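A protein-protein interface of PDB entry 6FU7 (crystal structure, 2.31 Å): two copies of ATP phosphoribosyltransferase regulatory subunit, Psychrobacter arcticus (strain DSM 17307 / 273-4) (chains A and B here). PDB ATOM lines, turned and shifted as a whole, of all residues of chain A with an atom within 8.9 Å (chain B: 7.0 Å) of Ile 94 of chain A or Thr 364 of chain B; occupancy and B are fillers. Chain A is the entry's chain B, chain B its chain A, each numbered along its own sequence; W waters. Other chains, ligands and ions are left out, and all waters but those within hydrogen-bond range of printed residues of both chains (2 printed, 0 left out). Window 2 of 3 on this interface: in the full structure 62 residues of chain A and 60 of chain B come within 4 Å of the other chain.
No position is printed for both chains.
Of the 12 pairs that touch across the chains among the printed residues, none has its exchanged pair printed and touching as well.
Hydrophobic or aromatic side chains of chain A within 4 Å of the printed part of chain B: Ile 94 and Ala 131.
Along chain A the printed residues that touch a printed residue of chain B span positions 35 to 135.
Printed residues of chain B that touch a printed residue of chain A: Met 361, Leu 363, Thr 364, Asp 367 and Val 370.
Hydrophobic or aromatic side chains of chain B that line the printed part of chain A: Leu 363 and Val 370.
Among the printed residues, Asp or Glu carboxylates within 4 Å of a Lys or Arg side-chain nitrogen of the other chain: Arg 96 of chain A with Asp 367 of chain B (2.8 Å).
Water W1 bridges OE1 of Glu 135 of chain A (2.5 Å) and O of Met 361 of chain B (2.6 Å).
Water W2 lies within hydrogen-bond range of the backbone NH (N) of Met 368 of chain B and the backbone carbonyl oxygen (O) of Ile 94 of chain A.
The side-chain carboxylate (OD2) of Asp 367 of chain B is in hydrogen-bond range of the backbone NH (N) of Leu 363 of chain B (2.9 Å).
N of Glu 366 of chain B sits close to OG1 of Thr 364 of chain B (3.4 Å).
N of Asp 367 of chain B sits at hydrogen-bond distance from OG1 of Thr 364 of chain B (3.2 Å).
OH of Tyr 34 of chain A sits at hydrogen-bond distance from OE2 of Glu 135 of chain A, at 2.9 Å.
SG of Cys 127 of chain A sits close to N of Ser 129 of chain A (3.6 Å).
N of Ala 131 of chain A sits close to OG of Ser 129 of chain A, at 3.1 Å.
Among the printed residues, pairs that only touch across the chains: Glu 135 of chain A with Leu 363 of chain B (3.4 Å), Ala 131 of chain A with Leu 363 of chain B (3.5 Å), Arg 96 of chain A with Leu 363 of chain B (3.5 Å), Gln 35 of chain A with Val 370 of chain B (3.5 Å), Glu 135 of chain A with Met 361 of chain B (3.7 Å), Ala 132 of chain A with Leu 363 of chain B (3.8 Å), Ile 94 of chain A with Thr 364 of chain B (3.9 Å), Ile 94 of chain A with Leu 363 of chain B (3.9 Å), Ile 94 of chain A with Asp 367 of chain B (3.95 Å) and Cys 127 of chain A with Leu 363 of chain B (3.95 Å).
The guanidinium group (NH2) of Arg 96 of chain A is in hydrogen-bond range of the backbone carbonyl oxygen (O) of Met 361 of chain B (3.3 Å).
NH2 of Arg 96 of chain A lies within salt-bridge range of OD2 of Asp 367 of chain B.
Of chain B, only Leu 363, Thr 364 and Asp 367 come within 4 Å of Ile 94 of chain A.
Of chain A, only Ile 94 comes within 4 Å of Thr 364 of chain B.
No residue of chain A comes within 4 Å of Ala 365 of chain B.
Printed residues of chain B within 4 Å of Ala 132 of chain A: Leu 363.
Of the printed residues of chain A, Met 361 of chain B touches Arg 96 and Glu 135.
Printed residues of chain B within 4 Å of Cys 127 of chain A: Leu 363.
Of the printed residues of chain B, Gln 35 of chain A touches Val 370 (3.5 Å).
Of the printed residues of chain A, Val 370 of chain B touches Gln 35.
Glu 366 of chain B touches none of the printed residues of chain A.
The nearest residue of chain B that does not touch Ile 94 of chain A is Met 368 of chain B (4.8 Å).
The nearest printed residue of chain B that does not touch Cys 127 of chain A is Thr 364 of chain B (5.1 Å).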
ATOM      1  N   GLY A  33      17.712  18.016  21.670  1.00  0.00           N
ATOM      2  CA  GLY A  33      17.512  17.103  22.789  1.00  0.00           C
ATOM      3  C   GLY A  33      17.814  17.706  24.150  1.00  0.00           C
ATOM      4  O   GLY A  33      17.975  16.975  25.114  1.00  0.00           O
ATOM      5  N   TYR A  34      17.883  19.027  24.253  1.00  0.00           N
ATOM      6  CA  TYR A  34      18.119  19.663  25.548  1.00  0.00           C
ATOM      7  C   TYR A  34      16.767  19.934  26.213  1.00  0.00           C
ATOM      8  O   TYR A  34      15.858  20.444  25.569  1.00  0.00           O
ATOM      9  CB  TYR A  34      18.942  20.951  25.357  1.00  0.00           C
ATOM     10  CG  TYR A  34      20.342  20.632  24.909  1.00  0.00           C
ATOM     11  CD1 TYR A  34      20.609  20.310  23.589  1.00  0.00           C
ATOM     12  CD2 TYR A  34      21.400  20.614  25.816  1.00  0.00           C
ATOM     13  CE1 TYR A  34      21.894  19.947  23.185  1.00  0.00           C
ATOM     14  CE2 TYR A  34      22.685  20.262  25.425  1.00  0.00           C
ATOM     15  CZ  TYR A  34      22.923  19.909  24.114  1.00  0.00           C
ATOM     16  OH  TYR A  34      24.186  19.583  23.685  1.00  0.00           O
ATOM     17  N   GLN A  35      16.627  19.573  27.484  1.00  0.00           N
ATOM     18  CA  GLN A  35      15.377  19.810  28.223  1.00  0.00           C
ATOM     19  C   GLN A  35      15.362  21.247  28.749  1.00  0.00           C
ATOM     20  O   GLN A  35      16.251  21.654  29.494  1.00  0.00           O
ATOM     21  CB  GLN A  35      15.260  18.878  29.427  1.00  0.00           C
ATOM     22  CG  GLN A  35      15.374  17.386  29.150  1.00  0.00           C
ATOM     23  CD  GLN A  35      15.513  16.607  30.447  1.00  0.00           C
ATOM     24  OE1 GLN A  35      14.529  16.072  30.943  1.00  0.00           O
ATOM     25  NE2 GLN A  35      16.733  16.580  31.030  1.00  0.00           N
ATOM     26  N   ASP A  86      19.643  19.325  38.261  1.00  0.00           N
ATOM     27  CA  ASP A  86      20.258  18.067  37.875  1.00  0.00           C
ATOM     28  C   ASP A  86      20.466  17.109  39.057  1.00  0.00           C
ATOM     29  O   ASP A  86      20.295  15.900  38.905  1.00  0.00           O
ATOM     30  CB  ASP A  86      21.594  18.281  37.159  1.00  0.00           C
ATOM     31  CG  ASP A  86      22.267  16.960  36.781  1.00  0.00           C
ATOM     32  OD1 ASP A  86      21.771  16.269  35.854  1.00  0.00           O
ATOM     33  OD2 ASP A  86      23.285  16.606  37.426  1.00  0.00           O
ATOM     34  N   HIS A  89      16.735  15.827  39.749  1.00  0.00           N
ATOM     35  CA  HIS A  89      16.074  15.125  38.622  1.00  0.00           C
ATOM     36  C   HIS A  89      16.977  14.340  37.663  1.00  0.00           C
ATOM     37  O   HIS A  89      16.486  13.495  36.935  1.00  0.00           O
ATOM     38  CB  HIS A  89      15.266  16.118  37.758  1.00  0.00           C
ATOM     39  CG  HIS A  89      14.176  16.822  38.497  1.00  0.00           C
ATOM     40  ND1 HIS A  89      14.384  18.019  39.151  1.00  0.00           N
ATOM     41  CD2 HIS A  89      12.867  16.514  38.674  1.00  0.00           C
ATOM     42  CE1 HIS A  89      13.248  18.412  39.709  1.00  0.00           C
ATOM     43  NE2 HIS A  89      12.315  17.516  39.432  1.00  0.00           N
ATOM     44  N   GLY A  90      18.280  14.603  37.646  1.00  0.00           N
ATOM     45  CA  GLY A  90      19.148  14.122  36.570  1.00  0.00           C
ATOM     46  C   GLY A  90      19.602  12.666  36.585  1.00  0.00           C
ATOM     47  O   GLY A  90      19.959  12.112  35.538  1.00  0.00           O
ATOM     48  N   GLY A  91      19.615  12.037  37.758  1.00  0.00           N
ATOM     49  CA  GLY A  91      20.167  10.690  37.888  1.00  0.00           C
ATOM     50  C   GLY A  91      21.677  10.617  37.681  1.00  0.00           C
ATOM     51  O   GLY A  91      22.380  11.613  37.799  1.00  0.00           O
ATOM     52  N   ASP A  92      22.158   9.412  37.371  1.00  0.00           N
ATOM     53  CA  ASP A  92      23.590   9.112  37.194  1.00  0.00           C
ATOM     54  C   ASP A  92      24.045   9.147  35.742  1.00  0.00           C
ATOM     55  O   ASP A  92      25.230   9.303  35.474  1.00  0.00           O
ATOM     56  CB  ASP A  92      23.912   7.723  37.759  1.00  0.00           C
ATOM     57  CG  ASP A  92      23.655   7.613  39.258  1.00  0.00           C
ATOM     58  OD1 ASP A  92      23.521   8.663  39.927  1.00  0.00           O
ATOM     59  OD2 ASP A  92      23.597   6.469  39.771  1.00  0.00           O
ATOM     60  N   GLY A  93      23.115   8.990  34.807  1.00  0.00           N
ATOM     61  CA  GLY A  93      23.434   8.959  33.392  1.00  0.00           C
ATOM     62  C   GLY A  93      23.590  10.346  32.821  1.00  0.00           C
ATOM     63  O   GLY A  93      23.780  11.317  33.547  1.00  0.00           O
ATOM     64  N   ILE A  94      23.524  10.417  31.496  1.00  0.00           N
ATOM     65  CA  ILE A  94      23.650  11.671  30.767  1.00  0.00           C
ATOM     66  C   ILE A  94      22.336  12.444  30.835  1.00  0.00           C
ATOM     67  O   ILE A  94      21.273  11.885  30.624  1.00  0.00           O
ATOM     68  CB  ILE A  94      24.100  11.427  29.309  1.00  0.00           C
ATOM     69  CG1 ILE A  94      25.503  10.793  29.327  1.00  0.00           C
ATOM     70  CG2 ILE A  94      24.108  12.737  28.508  1.00  0.00           C
ATOM     71  CD1 ILE A  94      26.010  10.358  27.974  1.00  0.00           C
ATOM     72  N   ALA A  95      22.435  13.730  31.155  1.00  0.00           N
ATOM     73  CA  ALA A  95      21.297  14.630  31.184  1.00  0.00           C
ATOM     74  C   ALA A  95      21.662  15.934  30.476  1.00  0.00           C
ATOM     75  O   ALA A  95      22.764  16.457  30.658  1.00  0.00           O
ATOM     76  CB  ALA A  95      20.902  14.906  32.618  1.00  0.00           C
ATOM     77  N   ARG A  96      20.739  16.442  29.665  1.00  0.00           N
ATOM     78  CA  ARG A  96      20.938  17.657  28.891  1.00  0.00           C
ATOM     79  C   ARG A  96      19.865  18.692  29.281  1.00  0.00           C
ATOM     80  O   ARG A  96      18.676  18.356  29.402  1.00  0.00           O
ATOM     81  CB  ARG A  96      20.840  17.371  27.387  1.00  0.00           C
ATOM     82  CG  ARG A  96      21.932  16.460  26.804  1.00  0.00           C
ATOM     83  CD  ARG A  96      21.645  16.239  25.336  1.00  0.00           C
ATOM     84  NE  ARG A  96      22.655  15.455  24.636  1.00  0.00           N
ATOM     85  CZ  ARG A  96      22.793  14.132  24.689  1.00  0.00           C
ATOM     86  NH1 ARG A  96      21.983  13.380  25.431  1.00  0.00           N
ATOM     87  NH2 ARG A  96      23.743  13.549  23.973  1.00  0.00           N
ATOM     88  N   TYR A  97      20.293  19.940  29.483  1.00  0.00           N
ATOM     89  CA  TYR A  97      19.435  21.034  29.912  1.00  0.00           C
ATOM     90  C   TYR A  97      19.729  22.274  29.091  1.00  0.00           C
ATOM     91  O   TYR A  97      20.879  22.509  28.681  1.00  0.00           O
ATOM     92  CB  TYR A  97      19.666  21.385  31.395  1.00  0.00           C
ATOM     93  CG  TYR A  97      19.584  20.200  32.323  1.00  0.00           C
ATOM     94  CD1 TYR A  97      18.364  19.767  32.806  1.00  0.00           C
ATOM     95  CD2 TYR A  97      20.741  19.501  32.714  1.00  0.00           C
ATOM     96  CE1 TYR A  97      18.276  18.669  33.650  1.00  0.00           C
ATOM     97  CE2 TYR A  97      20.656  18.414  33.581  1.00  0.00           C
ATOM     98  CZ  TYR A  97      19.418  18.001  34.034  1.00  0.00           C
ATOM     99  OH  TYR A  97      19.320  16.917  34.871  1.00  0.00           O
ATOM    100  N   GLU A 123      23.695  22.862  28.660  1.00  0.00           N
ATOM    101  CA  GLU A 123      24.603  22.114  29.512  1.00  0.00           C
ATOM    102  C   GLU A 123      24.364  20.603  29.408  1.00  0.00           C
ATOM    103  O   GLU A 123      23.201  20.164  29.329  1.00  0.00           O
ATOM    104  CB  GLU A 123      24.451  22.576  30.959  1.00  0.00           C
ATOM    105  CG  GLU A 123      25.289  23.823  31.272  1.00  0.00           C
ATOM    106  CD  GLU A 123      24.861  24.551  32.518  1.00  0.00           C
ATOM    107  OE1 GLU A 123      24.549  23.850  33.502  1.00  0.00           O
ATOM    108  OE2 GLU A 123      24.862  25.803  32.507  1.00  0.00           O
ATOM    109  N   ILE A 124      25.465  19.837  29.392  1.00  0.00           N
ATOM    110  CA  ILE A 124      25.461  18.361  29.383  1.00  0.00           C
ATOM    111  C   ILE A 124      26.170  17.879  30.636  1.00  0.00           C
ATOM    112  O   ILE A 124      27.321  18.268  30.878  1.00  0.00           O
ATOM    113  CB  ILE A 124      26.201  17.759  28.165  1.00  0.00           C
ATOM    114  CG1 ILE A 124      25.679  18.365  26.864  1.00  0.00           C
ATOM    115  CG2 ILE A 124      26.019  16.244  28.111  1.00  0.00           C
ATOM    116  CD1 ILE A 124      26.360  17.862  25.611  1.00  0.00           C
ATOM    117  N   PHE A 125      25.474  17.049  31.417  1.00  0.00           N
ATOM    118  CA  PHE A 125      25.987  16.455  32.650  1.00  0.00           C
ATOM    119  C   PHE A 125      26.164  14.962  32.438  1.00  0.00           C
ATOM    120  O   PHE A 125      25.391  14.358  31.691  1.00  0.00           O
ATOM    121  CB  PHE A 125      25.009  16.661  33.803  1.00  0.00           C
ATOM    122  CG  PHE A 125      24.966  18.074  34.334  1.00  0.00           C
ATOM    123  CD1 PHE A 125      24.444  19.111  33.572  1.00  0.00           C
ATOM    124  CD2 PHE A 125      25.447  18.366  35.609  1.00  0.00           C
ATOM    125  CE1 PHE A 125      24.426  20.407  34.056  1.00  0.00           C
ATOM    126  CE2 PHE A 125      25.418  19.658  36.100  1.00  0.00           C
ATOM    127  CZ  PHE A 125      24.903  20.689  35.319  1.00  0.00           C
ATOM    128  N   GLY A 126      27.172  14.364  33.091  1.00  0.00           N
ATOM    129  CA  GLY A 126      27.333  12.905  33.109  1.00  0.00           C
ATOM    130  C   GLY A 126      28.123  12.253  31.976  1.00  0.00           C
ATOM    131  O   GLY A 126      28.083  11.021  31.818  1.00  0.00           O
ATOM    132  N   CYS A 127      28.845  13.047  31.192  1.00  0.00           N
ATOM    133  CA  CYS A 127      29.735  12.543  30.145  1.00  0.00           C
ATOM    134  C   CYS A 127      31.151  13.124  30.303  1.00  0.00           C
ATOM    135  O   CYS A 127      31.346  14.328  30.203  1.00  0.00           O
ATOM    136  CB  CYS A 127      29.193  12.872  28.745  1.00  0.00           C
ATOM    137  SG  CYS A 127      30.188  12.120  27.414  1.00  0.00           S
ATOM    138  N   GLU A 128      32.132  12.253  30.529  1.00  0.00           N
ATOM    139  CA  GLU A 128      33.542  12.682  30.654  1.00  0.00           C
ATOM    140  C   GLU A 128      34.212  12.937  29.292  1.00  0.00           C
ATOM    141  O   GLU A 128      35.157  13.720  29.207  1.00  0.00           O
ATOM    142  CB  GLU A 128      34.381  11.686  31.475  1.00  0.00           C
ATOM    143  CG  GLU A 128      34.460  10.255  30.948  1.00  0.00           C
ATOM    144  CD  GLU A 128      33.478   9.311  31.646  1.00  0.00           C
ATOM    145  OE1 GLU A 128      32.260   9.631  31.638  1.00  0.00           O
ATOM    146  OE2 GLU A 128      33.911   8.260  32.194  1.00  0.00           O
ATOM    147  N   SER A 129      33.715  12.290  28.239  1.00  0.00           N
ATOM    148  CA  SER A 129      34.335  12.348  26.914  1.00  0.00           C
ATOM    149  C   SER A 129      34.324  13.749  26.277  1.00  0.00           C
ATOM    150  O   SER A 129      33.402  14.550  26.501  1.00  0.00           O
ATOM    151  CB  SER A 129      33.633  11.362  25.969  1.00  0.00           C
ATOM    152  OG  SER A 129      34.173  11.412  24.655  1.00  0.00           O
ATOM    153  N   ALA A 131      33.616  14.148  23.339  1.00  0.00           N
ATOM    154  CA  ALA A 131      32.433  14.086  22.498  1.00  0.00           C
ATOM    155  C   ALA A 131      31.252  14.973  22.984  1.00  0.00           C
ATOM    156  O   ALA A 131      30.485  15.485  22.151  1.00  0.00           O
ATOM    157  CB  ALA A 131      31.982  12.639  22.333  1.00  0.00           C
ATOM    158  N   ALA A 132      31.109  15.127  24.304  1.00  0.00           N
ATOM    159  CA  ALA A 132      30.105  16.037  24.884  1.00  0.00           C
ATOM    160  C   ALA A 132      30.423  17.497  24.569  1.00  0.00           C
ATOM    161  O   ALA A 132      29.520  18.268  24.253  1.00  0.00           O
ATOM    162  CB  ALA A 132      29.960  15.841  26.387  1.00  0.00           C
ATOM    163  N   GLU A 135      29.670  17.991  20.890  1.00  0.00           N
ATOM    164  CA  GLU A 135      28.231  18.137  20.666  1.00  0.00           C
ATOM    165  C   GLU A 135      27.757  19.560  20.973  1.00  0.00           C
ATOM    166  O   GLU A 135      26.986  20.137  20.199  1.00  0.00           O
ATOM    167  CB  GLU A 135      27.440  17.132  21.492  1.00  0.00           C
ATOM    168  CG  GLU A 135      25.947  17.170  21.213  1.00  0.00           C
ATOM    169  CD  GLU A 135      25.154  16.344  22.203  1.00  0.00           C
ATOM    170  OE1 GLU A 135      25.547  15.178  22.455  1.00  0.00           O
ATOM    171  OE2 GLU A 135      24.136  16.860  22.721  1.00  0.00           O
ATOM    172  N   ARG A 303      30.484  14.231  39.354  1.00  0.00           N
ATOM    173  CA  ARG A 303      29.615  14.358  38.179  1.00  0.00           C
ATOM    174  C   ARG A 303      30.167  15.376  37.194  1.00  0.00           C
ATOM    175  O   ARG A 303      30.362  16.538  37.539  1.00  0.00           O
ATOM    176  CB  ARG A 303      28.203  14.750  38.593  1.00  0.00           C
ATOM    177  CG  ARG A 303      27.182  14.718  37.457  1.00  0.00           C
ATOM    178  CD  ARG A 303      25.826  14.287  37.968  1.00  0.00           C
ATOM    179  NE  ARG A 303      24.769  14.496  36.976  1.00  0.00           N
ATOM    180  CZ  ARG A 303      24.383  13.633  36.031  1.00  0.00           C
ATOM    181  NH1 ARG A 303      24.957  12.450  35.877  1.00  0.00           N
ATOM    182  NH2 ARG A 303      23.398  13.981  35.208  1.00  0.00           N
ATOM    183  N   GLN A 304      30.410  14.908  35.973  1.00  0.00           N
ATOM    184  CA  GLN A 304      30.987  15.730  34.922  1.00  0.00           C
ATOM    185  C   GLN A 304      29.934  16.729  34.419  1.00  0.00           C
ATOM    186  O   GLN A 304      28.744  16.415  34.393  1.00  0.00           O
ATOM    187  CB  GLN A 304      31.454  14.866  33.743  1.00  0.00           C
ATOM    188  CG  GLN A 304      32.530  13.825  34.071  1.00  0.00           C
ATOM    189  CD  GLN A 304      33.903  14.428  34.315  1.00  0.00           C
ATOM    190  OE1 GLN A 304      34.415  15.223  33.517  1.00  0.00           O
ATOM    191  NE2 GLN A 304      34.509  14.056  35.440  1.00  0.00           N
ATOM    192  N   LEU B 328      15.768   9.023  19.262  1.00  0.00           N
ATOM    193  CA  LEU B 328      17.145   8.617  19.539  1.00  0.00           C
ATOM    194  C   LEU B 328      17.731   7.896  18.323  1.00  0.00           C
ATOM    195  O   LEU B 328      17.147   6.961  17.786  1.00  0.00           O
ATOM    196  CB  LEU B 328      17.219   7.690  20.773  1.00  0.00           C
ATOM    197  CG  LEU B 328      18.576   7.085  21.179  1.00  0.00           C
ATOM    198  CD1 LEU B 328      19.614   8.154  21.481  1.00  0.00           C
ATOM    199  CD2 LEU B 328      18.370   6.194  22.399  1.00  0.00           C
ATOM    200  N   ILE B 329      18.887   8.364  17.877  1.00  0.00           N
ATOM    201  CA  ILE B 329      19.645   7.693  16.835  1.00  0.00           C
ATOM    202  C   ILE B 329      20.366   6.491  17.463  1.00  0.00           C
ATOM    203  O   ILE B 329      20.874   6.581  18.574  1.00  0.00           O
ATOM    204  CB  ILE B 329      20.626   8.674  16.173  1.00  0.00           C
ATOM    205  CG1 ILE B 329      19.830   9.761  15.437  1.00  0.00           C
ATOM    206  CG2 ILE B 329      21.554   7.959  15.198  1.00  0.00           C
ATOM    207  CD1 ILE B 329      20.648  10.988  15.172  1.00  0.00           C
ATOM    208  N   TYR B 331      23.146   4.250  18.473  1.00  0.00           N
ATOM    209  CA  TYR B 331      24.572   4.507  18.721  1.00  0.00           C
ATOM    210  C   TYR B 331      25.478   3.648  17.837  1.00  0.00           C
ATOM    211  O   TYR B 331      26.361   4.169  17.139  1.00  0.00           O
ATOM    212  CB  TYR B 331      24.904   4.280  20.211  1.00  0.00           C
ATOM    213  CG  TYR B 331      26.356   4.490  20.575  1.00  0.00           C
ATOM    214  CD1 TYR B 331      26.901   5.775  20.638  1.00  0.00           C
ATOM    215  CD2 TYR B 331      27.187   3.408  20.853  1.00  0.00           C
ATOM    216  CE1 TYR B 331      28.232   5.972  20.963  1.00  0.00           C
ATOM    217  CE2 TYR B 331      28.523   3.594  21.192  1.00  0.00           C
ATOM    218  CZ  TYR B 331      29.038   4.878  21.245  1.00  0.00           C
ATOM    219  OH  TYR B 331      30.352   5.073  21.586  1.00  0.00           O
ATOM    220  N   MET B 361      21.572  12.872  19.267  1.00  0.00           N
ATOM    221  CA  MET B 361      22.768  12.142  18.815  1.00  0.00           C
ATOM    222  C   MET B 361      23.430  11.524  20.065  1.00  0.00           C
ATOM    223  O   MET B 361      23.951  12.262  20.914  1.00  0.00           O
ATOM    224  CB  MET B 361      23.780  13.097  18.147  1.00  0.00           C
ATOM    225  CG  MET B 361      23.285  13.902  16.953  1.00  0.00           C
ATOM    226  SD  MET B 361      22.903  12.982  15.449  1.00  0.00           S
ATOM    227  CE  MET B 361      24.197  11.730  15.315  1.00  0.00           C
ATOM    228  N   PRO B 362      23.415  10.188  20.203  1.00  0.00           N
ATOM    229  CA  PRO B 362      23.912   9.589  21.456  1.00  0.00           C
ATOM    230  C   PRO B 362      25.423   9.686  21.645  1.00  0.00           C
ATOM    231  O   PRO B 362      26.177   9.485  20.697  1.00  0.00           O
ATOM    232  CB  PRO B 362      23.492   8.126  21.330  1.00  0.00           C
ATOM    233  CG  PRO B 362      23.533   7.882  19.871  1.00  0.00           C
ATOM    234  CD  PRO B 362      23.014   9.150  19.238  1.00  0.00           C
ATOM    235  N   LEU B 363      25.847   9.991  22.865  1.00  0.00           N
ATOM    236  CA  LEU B 363      27.269  10.051  23.228  1.00  0.00           C
ATOM    237  C   LEU B 363      27.806   8.670  23.569  1.00  0.00           C
ATOM    238  O   LEU B 363      28.960   8.369  23.284  1.00  0.00           O
ATOM    239  CB  LEU B 363      27.478  10.995  24.412  1.00  0.00           C
ATOM    240  CG  LEU B 363      27.103  12.444  24.119  1.00  0.00           C
ATOM    241  CD1 LEU B 363      26.975  13.237  25.404  1.00  0.00           C
ATOM    242  CD2 LEU B 363      28.125  13.068  23.187  1.00  0.00           C
ATOM    243  N   THR B 364      26.957   7.854  24.189  1.00  0.00           N
ATOM    244  CA  THR B 364      27.264   6.474  24.562  1.00  0.00           C
ATOM    245  C   THR B 364      26.080   5.572  24.218  1.00  0.00           C
ATOM    246  O   THR B 364      24.973   6.043  23.936  1.00  0.00           O
ATOM    247  CB  THR B 364      27.522   6.353  26.072  1.00  0.00           C
ATOM    248  OG1 THR B 364      26.323   6.673  26.794  1.00  0.00           O
ATOM    249  CG2 THR B 364      28.632   7.296  26.505  1.00  0.00           C
ATOM    250  N   ALA B 365      26.319   4.269  24.301  1.00  0.00           N
ATOM    251  CA  ALA B 365      25.294   3.243  24.095  1.00  0.00           C
ATOM    252  C   ALA B 365      24.159   3.268  25.133  1.00  0.00           C
ATOM    253  O   ALA B 365      23.121   2.662  24.893  1.00  0.00           O
ATOM    254  CB  ALA B 365      25.946   1.854  24.075  1.00  0.00           C
ATOM    255  N   GLU B 366      24.346   3.951  26.253  1.00  0.00           N
ATOM    256  CA  GLU B 366      23.325   4.107  27.308  1.00  0.00           C
ATOM    257  C   GLU B 366      22.574   5.445  27.239  1.00  0.00           C
ATOM    258  O   GLU B 366      21.523   5.575  27.841  1.00  0.00           O
ATOM    259  CB  GLU B 366      23.885   3.889  28.741  1.00  0.00           C
ATOM    260  CG  GLU B 366      25.400   3.927  28.982  1.00  0.00           C
ATOM    261  CD  GLU B 366      26.173   2.824  28.286  1.00  0.00           C
ATOM    262  OE1 GLU B 366      25.627   1.724  28.039  1.00  0.00           O
ATOM    263  OE2 GLU B 366      27.359   3.082  27.987  1.00  0.00           O
ATOM    264  N   ASP B 367      23.120   6.421  26.517  1.00  0.00           N
ATOM    265  CA  ASP B 367      22.516   7.755  26.353  1.00  0.00           C
ATOM    266  C   ASP B 367      21.080   7.644  25.835  1.00  0.00           C
ATOM    267  O   ASP B 367      20.855   7.321  24.671  1.00  0.00           O
ATOM    268  CB  ASP B 367      23.382   8.593  25.393  1.00  0.00           C
ATOM    269  CG  ASP B 367      23.009  10.070  25.349  1.00  0.00           C
ATOM    270  OD1 ASP B 367      22.035  10.514  25.985  1.00  0.00           O
ATOM    271  OD2 ASP B 367      23.717  10.813  24.646  1.00  0.00           O
ATOM    272  N   MET B 368      20.123   7.904  26.726  1.00  0.00           N
ATOM    273  CA  MET B 368      18.702   7.831  26.408  1.00  0.00           C
ATOM    274  C   MET B 368      17.973   9.112  26.826  1.00  0.00           C
ATOM    275  O   MET B 368      18.009   9.475  28.002  1.00  0.00           O
ATOM    276  CB  MET B 368      18.098   6.655  27.148  1.00  0.00           C
ATOM    277  CG  MET B 368      16.715   6.274  26.644  1.00  0.00           C
ATOM    278  SD  MET B 368      16.454   4.518  26.862  1.00  0.00           S
ATOM    279  CE  MET B 368      17.758   3.799  25.853  1.00  0.00           C
ATOM    280  N   PRO B 369      17.301   9.805  25.879  1.00  0.00           N
ATOM    281  CA  PRO B 369      16.506  10.970  26.282  1.00  0.00           C
ATOM    282  C   PRO B 369      15.259  10.599  27.090  1.00  0.00           C
ATOM    283  O   PRO B 369      14.698   9.502  26.920  1.00  0.00           O
ATOM    284  CB  PRO B 369      16.102  11.600  24.949  1.00  0.00           C
ATOM    285  CG  PRO B 369      16.137  10.482  23.970  1.00  0.00           C
ATOM    286  CD  PRO B 369      17.251   9.594  24.421  1.00  0.00           C
ATOM    287  N   VAL B 370      14.845  11.521  27.958  1.00  0.00           N
ATOM    288  CA  VAL B 370      13.648  11.352  28.785  1.00  0.00           C
ATOM    289  C   VAL B 370      12.440  11.346  27.850  1.00  0.00           C
ATOM    290  O   VAL B 370      12.355  12.178  26.943  1.00  0.00           O
ATOM    291  CB  VAL B 370      13.493  12.494  29.836  1.00  0.00           C
ATOM    292  CG1 VAL B 370      12.189  12.351  30.622  1.00  0.00           C
ATOM    293  CG2 VAL B 370      14.683  12.536  30.798  1.00  0.00           C
HETATM  294  O   HOH W   1      26.095  13.639  20.569  1.00  0.00           O
HETATM  295  O   HOH W   2      21.077   8.821  29.415  1.00  0.00           O
